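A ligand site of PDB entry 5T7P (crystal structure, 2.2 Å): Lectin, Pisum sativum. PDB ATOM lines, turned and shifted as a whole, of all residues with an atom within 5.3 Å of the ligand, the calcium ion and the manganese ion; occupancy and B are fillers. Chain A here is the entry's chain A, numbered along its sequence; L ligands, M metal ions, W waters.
O3 of the ligand is in hydrogen-bond range of ND2 of Asn 125 (2.6 Å). The side-chain carboxylate (OD1) of Asp 81 lies within hydrogen-bond range of an oxygen (O3) of the ligand (2.6 Å). N of Ala 217 is in hydrogen-bond range of O4 of the ligand, 2.7 Å away. An oxygen (O5) of the ligand lies within hydrogen-bond range of the backbone NH of Gly 216 (2.9 Å). The backbone NH (N) of Gly 99 is in hydrogen-bond range of an oxygen (O2) of the ligand. N of Glu 218 is in hydrogen-bond range of O5 of the ligand (3.1 Å). O of Glu 218 sits at hydrogen-bond distance from O5 of the ligand, 3.2 Å away.
NE1 of Trp 128 lies close to OD1 of Asp 129 (3.5 Å). The side-chain carboxylate (OE1) of Glu 119 sits close to the side-chain hydroxyl (OG) of Ser 146 (3.4 Å). The side-chain carboxylate (OD2) of Asp 81 is in hydrogen-bond range of the backbone NH (N) of Gly 216 (2.9 Å). The backbone NH (N) of Gly 99 lies within hydrogen-bond range of the side-chain carboxylate (OD1) of Asp 81. The backbone NH (N) of Asn 39 lies within hydrogen-bond range of the backbone carbonyl oxygen (O) of Gly 216 (2.9 Å).
Residues that only touch the ligand: Ala 80 and Gly 98. Hydrophobic or aromatic side chains within 4 Å of the ligand: Ala 80, Phe 123 and Ala 217.
The nearest printed residue that does not touch the calcium ion is Trp 128 (4.2 Å).
The nearest printed residue that does not touch the manganese ion is Ser 146 (4.2 Å).
The calcium ion is bound by O of Phe 123 (2.3 Å), OD2 of Asp 129 (2.3 Å), water W2 (2.4 Å), OD1 of Asn 125 (2.4 Å), OD1 of Asp 121 (2.4 Å), water W5 (2.4 Å) and OD2 of Asp 121 (2.5 Å).
The side-chain carboxylate (OD2) of Asp 121 binds the manganese ion (2.1 Å). The manganese ion is bound by OD1 of Asp 129, 2.1 Å away. NE2 of His 136 binds the manganese ion (2.2 Å). The side-chain carboxylate (OE1) of Glu 119 is bound to the manganese ion (2.2 Å). Water W3 is bound to the manganese ion (2.3 Å). Water W1 is bound to the manganese ion (2.3 Å). The manganese ion has six donor atoms within binding distance.
Water W2 bridges the backbone carbonyl oxygen of Gly 99 (2.7 Å) and the indole nitrogen of Trp 128 (2.8 Å). Water W1 bridges the backbone carbonyl oxygen of Ile 144 (2.7 Å) and the indole nitrogen of Trp 128 (3.5 Å). Water W7 bridges a nitrogen (N1) of the ligand (2.7 Å) and the side-chain carboxylate (OE2) of Glu 218 (2.9 Å).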
ATOM      1  N   ASN A  39       8.528 -21.675  11.228  1.00  0.00           N
ATOM      2  CA  ASN A  39       8.700 -21.017  12.519  1.00  0.00           C
ATOM      3  C   ASN A  39       9.966 -21.458  13.240  1.00  0.00           C
ATOM      4  O   ASN A  39       9.959 -21.770  14.434  1.00  0.00           O
ATOM      5  CB  ASN A  39       7.485 -21.256  13.416  1.00  0.00           C
ATOM      6  CG  ASN A  39       6.234 -20.617  12.856  1.00  0.00           C
ATOM      7  OD1 ASN A  39       6.236 -19.436  12.525  1.00  0.00           O
ATOM      8  ND2 ASN A  39       5.184 -21.407  12.715  1.00  0.00           N
ATOM      9  N   ALA A  80      10.008 -17.687   2.624  1.00  0.00           N
ATOM     10  CA  ALA A  80      10.296 -16.961   3.857  1.00  0.00           C
ATOM     11  C   ALA A  80      11.337 -17.692   4.735  1.00  0.00           C
ATOM     12  O   ALA A  80      11.489 -18.882   4.654  1.00  0.00           O
ATOM     13  CB  ALA A  80       9.052 -16.622   4.645  1.00  0.00           C
ATOM     14  N   ASP A  81      12.013 -16.956   5.576  1.00  0.00           N
ATOM     15  CA  ASP A  81      11.900 -15.541   5.692  1.00  0.00           C
ATOM     16  C   ASP A  81      13.163 -14.895   5.171  1.00  0.00           C
ATOM     17  O   ASP A  81      13.181 -13.750   4.898  1.00  0.00           O
ATOM     18  CB  ASP A  81      11.752 -15.106   7.123  1.00  0.00           C
ATOM     19  CG  ASP A  81      10.359 -15.074   7.565  1.00  0.00           C
ATOM     20  OD1 ASP A  81       9.713 -14.141   7.262  1.00  0.00           O
ATOM     21  OD2 ASP A  81       9.911 -16.013   8.209  1.00  0.00           O
ATOM     22  N   GLY A  97      12.054 -14.267  15.831  1.00  0.00           N
ATOM     23  CA  GLY A  97      11.980 -15.135  14.676  1.00  0.00           C
ATOM     24  C   GLY A  97      11.204 -14.529  13.521  1.00  0.00           C
ATOM     25  O   GLY A  97      10.942 -13.320  13.475  1.00  0.00           O
ATOM     26  N   GLY A  98      10.847 -15.385  12.568  1.00  0.00           N
ATOM     27  CA  GLY A  98      10.016 -14.938  11.459  1.00  0.00           C
ATOM     28  C   GLY A  98      10.687 -13.808  10.702  1.00  0.00           C
ATOM     29  O   GLY A  98      11.897 -13.842  10.433  1.00  0.00           O
ATOM     30  N   GLY A  99       9.917 -12.778  10.374  1.00  0.00           N
ATOM     31  CA  GLY A  99      10.432 -11.647   9.616  1.00  0.00           C
ATOM     32  C   GLY A  99      11.548 -10.873  10.316  1.00  0.00           C
ATOM     33  O   GLY A  99      12.187 -10.032   9.678  1.00  0.00           O
ATOM     34  N   TYR A 100      11.782 -11.138  11.598  1.00  0.00           N
ATOM     35  CA  TYR A 100      12.875 -10.478  12.309  1.00  0.00           C
ATOM     36  C   TYR A 100      14.220 -11.150  12.101  1.00  0.00           C
ATOM     37  O   TYR A 100      15.229 -10.627  12.581  1.00  0.00           O
ATOM     38  CB  TYR A 100      12.539 -10.393  13.807  1.00  0.00           C
ATOM     39  CG  TYR A 100      11.430  -9.419  14.097  1.00  0.00           C
ATOM     40  CD1 TYR A 100      10.098  -9.831  14.078  1.00  0.00           C
ATOM     41  CD2 TYR A 100      11.716  -8.064  14.346  1.00  0.00           C
ATOM     42  CE1 TYR A 100       9.071  -8.923  14.317  1.00  0.00           C
ATOM     43  CE2 TYR A 100      10.712  -7.164  14.583  1.00  0.00           C
ATOM     44  CZ  TYR A 100       9.386  -7.595  14.573  1.00  0.00           C
ATOM     45  OH  TYR A 100       8.382  -6.696  14.810  1.00  0.00           O
ATOM     46  N   GLU A 119      20.862  -8.393   5.074  1.00  0.00           N
ATOM     47  CA  GLU A 119      19.745  -9.315   4.971  1.00  0.00           C
ATOM     48  C   GLU A 119      19.486  -9.647   3.511  1.00  0.00           C
ATOM     49  O   GLU A 119      19.673  -8.810   2.615  1.00  0.00           O
ATOM     50  CB  GLU A 119      18.468  -8.758   5.631  1.00  0.00           C
ATOM     51  CG  GLU A 119      17.963  -7.398   5.124  1.00  0.00           C
ATOM     52  CD  GLU A 119      16.523  -7.096   5.527  1.00  0.00           C
ATOM     53  OE1 GLU A 119      15.681  -6.848   4.642  1.00  0.00           O
ATOM     54  OE2 GLU A 119      16.218  -7.117   6.731  1.00  0.00           O
ATOM     55  N   ASP A 121      16.271 -10.943   2.130  1.00  0.00           N
ATOM     56  CA  ASP A 121      14.946 -11.008   2.752  1.00  0.00           C
ATOM     57  C   ASP A 121      13.928 -11.449   1.703  1.00  0.00           C
ATOM     58  O   ASP A 121      13.636 -10.694   0.763  1.00  0.00           O
ATOM     59  CB  ASP A 121      14.596  -9.629   3.333  1.00  0.00           C
ATOM     60  CG  ASP A 121      13.255  -9.594   4.027  1.00  0.00           C
ATOM     61  OD1 ASP A 121      12.446 -10.532   3.876  1.00  0.00           O
ATOM     62  OD2 ASP A 121      12.992  -8.605   4.711  1.00  0.00           O
ATOM     63  N   PHE A 123      10.636 -12.411   2.175  1.00  0.00           N
ATOM     64  CA  PHE A 123       9.225 -12.297   2.526  1.00  0.00           C
ATOM     65  C   PHE A 123       8.869 -10.865   2.912  1.00  0.00           C
ATOM     66  O   PHE A 123       9.485 -10.281   3.799  1.00  0.00           O
ATOM     67  CB  PHE A 123       8.857 -13.231   3.682  1.00  0.00           C
ATOM     68  CG  PHE A 123       7.389 -13.244   3.992  1.00  0.00           C
ATOM     69  CD1 PHE A 123       6.511 -14.082   3.305  1.00  0.00           C
ATOM     70  CD2 PHE A 123       6.862 -12.398   4.975  1.00  0.00           C
ATOM     71  CE1 PHE A 123       5.146 -14.083   3.598  1.00  0.00           C
ATOM     72  CE2 PHE A 123       5.491 -12.391   5.267  1.00  0.00           C
ATOM     73  CZ  PHE A 123       4.642 -13.233   4.585  1.00  0.00           C
ATOM     74  N   TYR A 124       7.826 -10.339   2.285  1.00  0.00           N
ATOM     75  CA  TYR A 124       7.380  -8.973   2.506  1.00  0.00           C
ATOM     76  C   TYR A 124       6.647  -8.878   3.839  1.00  0.00           C
ATOM     77  O   TYR A 124       5.514  -9.342   3.978  1.00  0.00           O
ATOM     78  CB  TYR A 124       6.487  -8.522   1.360  1.00  0.00           C
ATOM     79  CG  TYR A 124       5.790  -7.198   1.628  1.00  0.00           C
ATOM     80  CD1 TYR A 124       6.512  -6.017   1.638  1.00  0.00           C
ATOM     81  CD2 TYR A 124       4.403  -7.142   1.868  1.00  0.00           C
ATOM     82  CE1 TYR A 124       5.899  -4.805   1.887  1.00  0.00           C
ATOM     83  CE2 TYR A 124       3.767  -5.910   2.110  1.00  0.00           C
ATOM     84  CZ  TYR A 124       4.540  -4.742   2.110  1.00  0.00           C
ATOM     85  OH  TYR A 124       3.961  -3.519   2.347  1.00  0.00           O
ATOM     86  N   ASN A 125       7.284  -8.265   4.829  1.00  0.00           N
ATOM     87  CA  ASN A 125       6.596  -7.918   6.073  1.00  0.00           C
ATOM     88  C   ASN A 125       6.084  -6.496   5.932  1.00  0.00           C
ATOM     89  O   ASN A 125       6.878  -5.547   5.862  1.00  0.00           O
ATOM     90  CB  ASN A 125       7.524  -8.074   7.271  1.00  0.00           C
ATOM     91  CG  ASN A 125       7.989  -9.505   7.452  1.00  0.00           C
ATOM     92  OD1 ASN A 125       9.043  -9.885   6.955  1.00  0.00           O
ATOM     93  ND2 ASN A 125       7.161 -10.320   8.119  1.00  0.00           N
ATOM     94  N   TRP A 128       7.336  -3.086   7.765  1.00  0.00           N
ATOM     95  CA  TRP A 128       8.619  -2.395   7.595  1.00  0.00           C
ATOM     96  C   TRP A 128       9.291  -2.571   6.239  1.00  0.00           C
ATOM     97  O   TRP A 128      10.166  -1.766   5.903  1.00  0.00           O
ATOM     98  CB  TRP A 128       9.608  -2.842   8.654  1.00  0.00           C
ATOM     99  CG  TRP A 128       9.844  -4.325   8.689  1.00  0.00           C
ATOM    100  CD1 TRP A 128      10.617  -5.057   7.854  1.00  0.00           C
ATOM    101  CD2 TRP A 128       9.296  -5.256   9.640  1.00  0.00           C
ATOM    102  NE1 TRP A 128      10.593  -6.388   8.206  1.00  0.00           N
ATOM    103  CE2 TRP A 128       9.791  -6.540   9.309  1.00  0.00           C
ATOM    104  CE3 TRP A 128       8.437  -5.143  10.733  1.00  0.00           C
ATOM    105  CZ2 TRP A 128       9.452  -7.682  10.023  1.00  0.00           C
ATOM    106  CZ3 TRP A 128       8.093  -6.288  11.455  1.00  0.00           C
ATOM    107  CH2 TRP A 128       8.610  -7.533  11.104  1.00  0.00           C
ATOM    108  N   ASP A 129       8.957  -3.627   5.492  1.00  0.00           N
ATOM    109  CA  ASP A 129       9.711  -3.938   4.282  1.00  0.00           C
ATOM    110  C   ASP A 129       9.386  -2.965   3.150  1.00  0.00           C
ATOM    111  O   ASP A 129       8.343  -2.316   3.176  1.00  0.00           O
ATOM    112  CB  ASP A 129       9.449  -5.377   3.860  1.00  0.00           C
ATOM    113  CG  ASP A 129      10.431  -6.338   4.484  1.00  0.00           C
ATOM    114  OD1 ASP A 129      11.507  -5.855   4.876  1.00  0.00           O
ATOM    115  OD2 ASP A 129      10.132  -7.561   4.603  1.00  0.00           O
ATOM    116  N   PRO A 130      10.260  -2.858   2.151  1.00  0.00           N
ATOM    117  CA  PRO A 130      10.019  -1.898   1.055  1.00  0.00           C
ATOM    118  C   PRO A 130       8.668  -2.139   0.412  1.00  0.00           C
ATOM    119  O   PRO A 130       8.237  -3.277   0.215  1.00  0.00           O
ATOM    120  CB  PRO A 130      11.171  -2.169   0.084  1.00  0.00           C
ATOM    121  CG  PRO A 130      12.270  -2.701   0.948  1.00  0.00           C
ATOM    122  CD  PRO A 130      11.563  -3.546   1.998  1.00  0.00           C
ATOM    123  N   HIS A 136      14.465  -8.585  -1.355  1.00  0.00           N
ATOM    124  CA  HIS A 136      15.414  -7.477  -1.330  1.00  0.00           C
ATOM    125  C   HIS A 136      16.607  -7.808  -0.470  1.00  0.00           C
ATOM    126  O   HIS A 136      16.506  -8.508   0.543  1.00  0.00           O
ATOM    127  CB  HIS A 136      14.761  -6.190  -0.821  1.00  0.00           C
ATOM    128  CG  HIS A 136      14.095  -6.353   0.505  1.00  0.00           C
ATOM    129  ND1 HIS A 136      12.822  -6.867   0.632  1.00  0.00           N
ATOM    130  CD2 HIS A 136      14.516  -6.083   1.763  1.00  0.00           C
ATOM    131  CE1 HIS A 136      12.489  -6.883   1.909  1.00  0.00           C
ATOM    132  NE2 HIS A 136      13.499  -6.416   2.608  1.00  0.00           N
ATOM    133  N   ILE A 144      15.040  -4.032  12.091  1.00  0.00           N
ATOM    134  CA  ILE A 144      14.656  -4.885  10.969  1.00  0.00           C
ATOM    135  C   ILE A 144      14.225  -4.061   9.766  1.00  0.00           C
ATOM    136  O   ILE A 144      14.026  -4.600   8.674  1.00  0.00           O
ATOM    137  CB  ILE A 144      13.538  -5.859  11.376  1.00  0.00           C
ATOM    138  CG1 ILE A 144      13.450  -7.063  10.421  1.00  0.00           C
ATOM    139  CG2 ILE A 144      12.191  -5.130  11.430  1.00  0.00           C
ATOM    140  CD1 ILE A 144      14.804  -7.743  10.113  1.00  0.00           C
ATOM    141  N   SER A 146      15.490  -1.838   7.129  1.00  0.00           N
ATOM    142  CA  SER A 146      16.801  -1.562   6.591  1.00  0.00           C
ATOM    143  C   SER A 146      16.991  -0.063   6.331  1.00  0.00           C
ATOM    144  O   SER A 146      16.069   0.612   5.874  1.00  0.00           O
ATOM    145  CB  SER A 146      17.010  -2.331   5.281  1.00  0.00           C
ATOM    146  OG  SER A 146      16.641  -3.713   5.412  1.00  0.00           O
ATOM    147  N   THR A 215      12.455 -18.959   9.346  1.00  0.00           N
ATOM    148  CA  THR A 215      11.199 -19.195   8.666  1.00  0.00           C
ATOM    149  C   THR A 215      10.080 -18.803   9.610  1.00  0.00           C
ATOM    150  O   THR A 215      10.286 -18.685  10.814  1.00  0.00           O
ATOM    151  CB  THR A 215      11.062 -20.644   8.283  1.00  0.00           C
ATOM    152  OG1 THR A 215      11.014 -21.401   9.495  1.00  0.00           O
ATOM    153  CG2 THR A 215      12.269 -21.081   7.477  1.00  0.00           C
ATOM    154  N   GLY A 216       8.873 -18.635   9.063  1.00  0.00           N
ATOM    155  CA  GLY A 216       7.738 -18.293   9.898  1.00  0.00           C
ATOM    156  C   GLY A 216       6.535 -19.123   9.524  1.00  0.00           C
ATOM    157  O   GLY A 216       6.585 -20.358   9.599  1.00  0.00           O
ATOM    158  N   ALA A 217       5.437 -18.472   9.121  1.00  0.00           N
ATOM    159  CA  ALA A 217       4.314 -19.211   8.547  1.00  0.00           C
ATOM    160  C   ALA A 217       4.652 -19.757   7.166  1.00  0.00           C
ATOM    161  O   ALA A 217       4.050 -20.751   6.730  1.00  0.00           O
ATOM    162  CB  ALA A 217       3.074 -18.336   8.480  1.00  0.00           C
ATOM    163  N   GLU A 218       5.591 -19.134   6.461  1.00  0.00           N
ATOM    164  CA  GLU A 218       6.181 -19.671   5.249  1.00  0.00           C
ATOM    165  C   GLU A 218       7.630 -20.028   5.540  1.00  0.00           C
ATOM    166  O   GLU A 218       8.171 -19.677   6.582  1.00  0.00           O
ATOM    167  CB  GLU A 218       6.032 -18.684   4.085  1.00  0.00           C
ATOM    168  CG  GLU A 218       4.565 -18.388   3.793  1.00  0.00           C
ATOM    169  CD  GLU A 218       4.352 -17.448   2.617  1.00  0.00           C
ATOM    170  OE1 GLU A 218       5.314 -17.163   1.882  1.00  0.00           O
ATOM    171  OE2 GLU A 218       3.214 -16.992   2.433  1.00  0.00           O
ATOM    172  N   TYR A 219       8.235 -20.792   4.644  1.00  0.00           N
ATOM    173  CA  TYR A 219       9.485 -21.447   5.006  1.00  0.00           C
ATOM    174  C   TYR A 219      10.277 -21.781   3.759  1.00  0.00           C
ATOM    175  O   TYR A 219       9.778 -21.713   2.637  1.00  0.00           O
ATOM    176  CB  TYR A 219       9.228 -22.688   5.856  1.00  0.00           C
ATOM    177  CG  TYR A 219       8.366 -23.711   5.176  1.00  0.00           C
ATOM    178  CD1 TYR A 219       6.971 -23.639   5.251  1.00  0.00           C
ATOM    179  CD2 TYR A 219       8.933 -24.755   4.462  1.00  0.00           C
ATOM    180  CE1 TYR A 219       6.166 -24.595   4.625  1.00  0.00           C
ATOM    181  CE2 TYR A 219       8.146 -25.712   3.834  1.00  0.00           C
ATOM    182  CZ  TYR A 219       6.758 -25.623   3.922  1.00  0.00           C
ATOM    183  OH  TYR A 219       5.999 -26.584   3.284  1.00  0.00           O
HETATM  184  O1  LIG L   1       6.035 -15.182  11.492  1.00  0.00           O
HETATM  185  C1  LIG L   1       5.222 -14.326  10.691  1.00  0.00           C
HETATM  186  C2  LIG L   1       6.106 -13.302   9.987  1.00  0.00           C
HETATM  187  O2  LIG L   1       6.983 -12.691  10.942  1.00  0.00           O
HETATM  188  C3  LIG L   1       6.925 -13.945   8.877  1.00  0.00           C
HETATM  189  O3  LIG L   1       7.564 -12.935   8.097  1.00  0.00           O
HETATM  190  C4  LIG L   1       6.039 -14.805   7.971  1.00  0.00           C
HETATM  191  O4  LIG L   1       5.342 -15.769   8.760  1.00  0.00           O
HETATM  192  C5  LIG L   1       6.867 -15.513   6.915  1.00  0.00           C
HETATM  193  O5  LIG L   1       7.340 -16.761   7.437  1.00  0.00           O
HETATM  194  C6  LIG L   1       4.437 -15.154   9.674  1.00  0.00           C
HETATM  195  O6  LIG L   1       3.539 -14.320   8.960  1.00  0.00           O
HETATM  196  C7  LIG L   1       2.489 -14.863   8.279  1.00  0.00           C
HETATM  197  C8  LIG L   1       1.214 -15.247   8.894  1.00  0.00           C
HETATM  198  C9  LIG L   1       0.473 -15.765   7.713  1.00  0.00           C
HETATM  199  N1  LIG L   1       1.271 -15.652   6.628  1.00  0.00           N
HETATM  200  C10 LIG L   1       2.500 -15.112   6.916  1.00  0.00           C
HETATM  201  C11 LIG L   1       0.584 -15.250  10.225  1.00  0.00           C
HETATM  202 CL1  LIG L   1       1.442 -14.632  11.679  1.00  0.00          CL
HETATM  203  C12 LIG L   1      -0.797 -15.779  10.313  1.00  0.00           C
HETATM  204 BR1  LIG L   1      -1.705 -15.825  11.979  1.00  0.00          BR
HETATM  205  C13 LIG L   1      -1.430 -16.246   9.161  1.00  0.00           C
HETATM  206  C14 LIG L   1      -0.823 -16.246   7.903  1.00  0.00           C
HETATM  207 CA    CA M   1      10.865  -9.585   5.450  1.00  0.00          CA
HETATM  208 MN    MN M   2      13.538  -6.544   4.765  1.00  0.00          MN
HETATM  209  O   HOH W   1      13.879  -6.690   7.047  1.00  0.00           O
HETATM  210  O   HOH W   2      11.923  -8.683   7.377  1.00  0.00           O
HETATM  211  O   HOH W   3      14.163  -4.329   4.900  1.00  0.00           O
HETATM  212  O   HOH W   4       5.702 -10.278  11.665  1.00  0.00           O
HETATM  213  O   HOH W   5      11.162 -11.921   6.041  1.00  0.00           O
HETATM  214  O   HOH W   6       2.657 -11.601   9.658  1.00  0.00           O
HETATM  215  O   HOH W   7       1.033 -17.242   4.400  1.00  0.00           O
